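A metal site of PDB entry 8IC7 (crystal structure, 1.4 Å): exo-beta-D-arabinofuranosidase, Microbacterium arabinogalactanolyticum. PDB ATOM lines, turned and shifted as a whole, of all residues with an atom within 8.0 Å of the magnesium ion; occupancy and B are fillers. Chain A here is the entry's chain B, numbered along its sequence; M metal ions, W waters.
The nearest printed residue that does not touch the magnesium ion is His 546 (4.2 Å).
Water W1 lies within hydrogen-bond range of OD2 of Asp 549 (2.7 Å) and OD2 of Asp 547 (2.7 Å).
OD2 of Asp 545 lies within hydrogen-bond range of N of Gly 550.
O of Trp 544 lies within hydrogen-bond range of N of Asp 553 (2.8 Å).
N of Gly 548 sits close to OD1 of Asp 545.
The side-chain carboxylate (OD1) of Asp 553 sits at hydrogen-bond distance from a ring nitrogen (ND1) of His 546 (2.9 Å).
The magnesium ion is bound by the side-chain carboxylate of Asp 545, the side-chain carboxylate of Asp 549, water W1, the side-chain carboxylate of Asp 553, the side-chain carboxylate of Asp 547 and the backbone carbonyl oxygen of Leu 551.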
ATOM      1  N   ALA A 541       0.593  26.321   3.237  1.00  0.00           N
ATOM      2  CA  ALA A 541      -0.498  27.108   2.666  1.00  0.00           C
ATOM      3  C   ALA A 541       0.075  28.303   1.886  1.00  0.00           C
ATOM      4  O   ALA A 541      -0.468  28.686   0.864  1.00  0.00           O
ATOM      5  CB  ALA A 541      -1.459  27.563   3.739  1.00  0.00           C
ATOM      6  N   TRP A 544       2.649  26.482  -1.342  1.00  0.00           N
ATOM      7  CA  TRP A 544       2.197  25.380  -2.185  1.00  0.00           C
ATOM      8  C   TRP A 544       0.749  25.539  -2.615  1.00  0.00           C
ATOM      9  O   TRP A 544       0.191  24.614  -3.175  1.00  0.00           O
ATOM     10  CB  TRP A 544       2.411  24.042  -1.474  1.00  0.00           C
ATOM     11  CG  TRP A 544       3.849  23.646  -1.353  1.00  0.00           C
ATOM     12  CD1 TRP A 544       4.827  23.872  -2.275  1.00  0.00           C
ATOM     13  CD2 TRP A 544       4.418  22.833  -0.320  1.00  0.00           C
ATOM     14  NE1 TRP A 544       6.001  23.299  -1.850  1.00  0.00           N
ATOM     15  CE2 TRP A 544       5.771  22.642  -0.663  1.00  0.00           C
ATOM     16  CE3 TRP A 544       3.932  22.230   0.841  1.00  0.00           C
ATOM     17  CZ2 TRP A 544       6.629  21.875   0.120  1.00  0.00           C
ATOM     18  CZ3 TRP A 544       4.806  21.521   1.654  1.00  0.00           C
ATOM     19  CH2 TRP A 544       6.131  21.362   1.290  1.00  0.00           C
ATOM     20  N   ASP A 545       0.125  26.694  -2.366  1.00  0.00           N
ATOM     21  CA  ASP A 545      -1.183  26.961  -2.939  1.00  0.00           C
ATOM     22  C   ASP A 545      -1.023  28.219  -3.781  1.00  0.00           C
ATOM     23  O   ASP A 545      -0.740  29.273  -3.220  1.00  0.00           O
ATOM     24  CB  ASP A 545      -2.220  27.132  -1.835  1.00  0.00           C
ATOM     25  CG  ASP A 545      -3.637  27.482  -2.275  1.00  0.00           C
ATOM     26  OD1 ASP A 545      -4.014  27.209  -3.409  1.00  0.00           O
ATOM     27  OD2 ASP A 545      -4.386  27.994  -1.406  1.00  0.00           O
ATOM     28  N   HIS A 546      -1.177  28.083  -5.098  1.00  0.00           N
ATOM     29  CA  HIS A 546      -0.870  29.196  -5.997  1.00  0.00           C
ATOM     30  C   HIS A 546      -2.115  29.835  -6.594  1.00  0.00           C
ATOM     31  O   HIS A 546      -2.001  30.767  -7.375  1.00  0.00           O
ATOM     32  CB  HIS A 546      -0.010  28.673  -7.150  1.00  0.00           C
ATOM     33  CG  HIS A 546       1.273  28.095  -6.681  1.00  0.00           C
ATOM     34  ND1 HIS A 546       1.443  26.734  -6.450  1.00  0.00           N
ATOM     35  CD2 HIS A 546       2.369  28.698  -6.278  1.00  0.00           C
ATOM     36  CE1 HIS A 546       2.683  26.548  -6.016  1.00  0.00           C
ATOM     37  NE2 HIS A 546       3.254  27.725  -5.885  1.00  0.00           N
ATOM     38  N   ASP A 547      -3.306  29.317  -6.301  1.00  0.00           N
ATOM     39  CA  ASP A 547      -4.527  29.771  -6.935  1.00  0.00           C
ATOM     40  C   ASP A 547      -5.510  30.179  -5.846  1.00  0.00           C
ATOM     41  O   ASP A 547      -6.679  30.346  -6.140  1.00  0.00           O
ATOM     42  CB  ASP A 547      -5.038  28.697  -7.898  1.00  0.00           C
ATOM     43  CG  ASP A 547      -5.256  27.353  -7.228  1.00  0.00           C
ATOM     44  OD1 ASP A 547      -5.253  27.344  -5.998  1.00  0.00           O
ATOM     45  OD2 ASP A 547      -5.439  26.322  -7.944  1.00  0.00           O
ATOM     46  N   GLY A 548      -5.000  30.262  -4.601  1.00  0.00           N
ATOM     47  CA  GLY A 548      -5.712  30.759  -3.432  1.00  0.00           C
ATOM     48  C   GLY A 548      -6.974  29.984  -3.032  1.00  0.00           C
ATOM     49  O   GLY A 548      -7.873  30.557  -2.408  1.00  0.00           O
ATOM     50  N   ASP A 549      -7.086  28.704  -3.382  1.00  0.00           N
ATOM     51  CA  ASP A 549      -8.317  27.975  -3.090  1.00  0.00           C
ATOM     52  C   ASP A 549      -8.219  27.183  -1.791  1.00  0.00           C
ATOM     53  O   ASP A 549      -9.187  26.525  -1.432  1.00  0.00           O
ATOM     54  CB  ASP A 549      -8.738  27.049  -4.224  1.00  0.00           C
ATOM     55  CG  ASP A 549      -7.729  25.954  -4.580  1.00  0.00           C
ATOM     56  OD1 ASP A 549      -6.651  25.959  -3.975  1.00  0.00           O
ATOM     57  OD2 ASP A 549      -8.037  25.155  -5.460  1.00  0.00           O
ATOM     58  N   GLY A 550      -7.054  27.190  -1.136  1.00  0.00           N
ATOM     59  CA  GLY A 550      -6.821  26.356   0.044  1.00  0.00           C
ATOM     60  C   GLY A 550      -6.247  24.957  -0.252  1.00  0.00           C
ATOM     61  O   GLY A 550      -5.767  24.325   0.693  1.00  0.00           O
ATOM     62  N   LEU A 551      -6.320  24.540  -1.498  1.00  0.00           N
ATOM     63  CA  LEU A 551      -5.812  23.246  -1.951  1.00  0.00           C
ATOM     64  C   LEU A 551      -4.385  23.480  -2.422  1.00  0.00           C
ATOM     65  O   LEU A 551      -4.115  24.390  -3.199  1.00  0.00           O
ATOM     66  CB  LEU A 551      -6.657  22.644  -3.077  1.00  0.00           C
ATOM     67  CG  LEU A 551      -8.081  22.245  -2.708  1.00  0.00           C
ATOM     68  CD1 LEU A 551      -8.849  21.687  -3.900  1.00  0.00           C
ATOM     69  CD2 LEU A 551      -8.080  21.268  -1.521  1.00  0.00           C
ATOM     70  N   LEU A 552      -3.449  22.624  -1.963  1.00  0.00           N
ATOM     71  CA  LEU A 552      -2.087  22.650  -2.463  1.00  0.00           C
ATOM     72  C   LEU A 552      -2.103  22.160  -3.926  1.00  0.00           C
ATOM     73  O   LEU A 552      -2.816  21.216  -4.282  1.00  0.00           O
ATOM     74  CB  LEU A 552      -1.216  21.750  -1.572  1.00  0.00           C
ATOM     75  CG  LEU A 552      -1.278  21.985  -0.063  1.00  0.00           C
ATOM     76  CD1 LEU A 552      -0.236  21.101   0.653  1.00  0.00           C
ATOM     77  CD2 LEU A 552      -1.054  23.467   0.277  1.00  0.00           C
ATOM     78  N   ASP A 553      -1.358  22.845  -4.771  1.00  0.00           N
ATOM     79  CA  ASP A 553      -1.476  22.717  -6.205  1.00  0.00           C
ATOM     80  C   ASP A 553      -0.108  22.962  -6.819  1.00  0.00           C
ATOM     81  O   ASP A 553       0.776  23.571  -6.220  1.00  0.00           O
ATOM     82  CB  ASP A 553      -2.541  23.671  -6.770  1.00  0.00           C
ATOM     83  CG  ASP A 553      -2.175  25.118  -6.478  1.00  0.00           C
ATOM     84  OD1 ASP A 553      -1.189  25.602  -7.087  1.00  0.00           O
ATOM     85  OD2 ASP A 553      -2.834  25.745  -5.561  1.00  0.00           O
ATOM     86  N   GLY A 554       0.060  22.448  -8.046  1.00  0.00           N
ATOM     87  CA  GLY A 554       1.303  22.617  -8.769  1.00  0.00           C
ATOM     88  C   GLY A 554       2.381  21.651  -8.290  1.00  0.00           C
ATOM     89  O   GLY A 554       2.102  20.697  -7.550  1.00  0.00           O
ATOM     90  N   GLY A 566      -0.866  19.690 -10.980  1.00  0.00           N
ATOM     91  CA  GLY A 566      -2.283  19.830 -10.729  1.00  0.00           C
ATOM     92  C   GLY A 566      -2.621  19.920  -9.237  1.00  0.00           C
ATOM     93  O   GLY A 566      -1.865  20.500  -8.471  1.00  0.00           O
ATOM     94  N   VAL A 567      -3.775  19.326  -8.901  1.00  0.00           N
ATOM     95  CA  VAL A 567      -4.282  19.287  -7.542  1.00  0.00           C
ATOM     96  C   VAL A 567      -4.671  17.842  -7.245  1.00  0.00           C
ATOM     97  O   VAL A 567      -5.480  17.246  -7.966  1.00  0.00           O
ATOM     98  CB  VAL A 567      -5.527  20.200  -7.350  1.00  0.00           C
ATOM     99  CG1 VAL A 567      -5.636  20.573  -5.891  1.00  0.00           C
ATOM    100  CG2 VAL A 567      -5.489  21.446  -8.207  1.00  0.00           C
ATOM    101  N   ASN A 572      -2.936  16.912  -0.315  1.00  0.00           N
ATOM    102  CA  ASN A 572      -3.989  17.701   0.310  1.00  0.00           C
ATOM    103  C   ASN A 572      -4.569  17.023   1.533  1.00  0.00           C
ATOM    104  O   ASN A 572      -4.915  17.719   2.510  1.00  0.00           O
ATOM    105  CB  ASN A 572      -5.037  18.033  -0.731  1.00  0.00           C
ATOM    106  CG  ASN A 572      -4.589  19.245  -1.520  1.00  0.00           C
ATOM    107  OD1 ASN A 572      -4.572  20.325  -0.946  1.00  0.00           O
ATOM    108  ND2 ASN A 572      -4.258  19.101  -2.795  1.00  0.00           N
HETATM  109 MG    MG M   1      -4.712  25.807  -4.652  1.00  0.00          MG
HETATM  110  O   HOH W   1      -5.536  24.475  -6.017  1.00  0.00           O
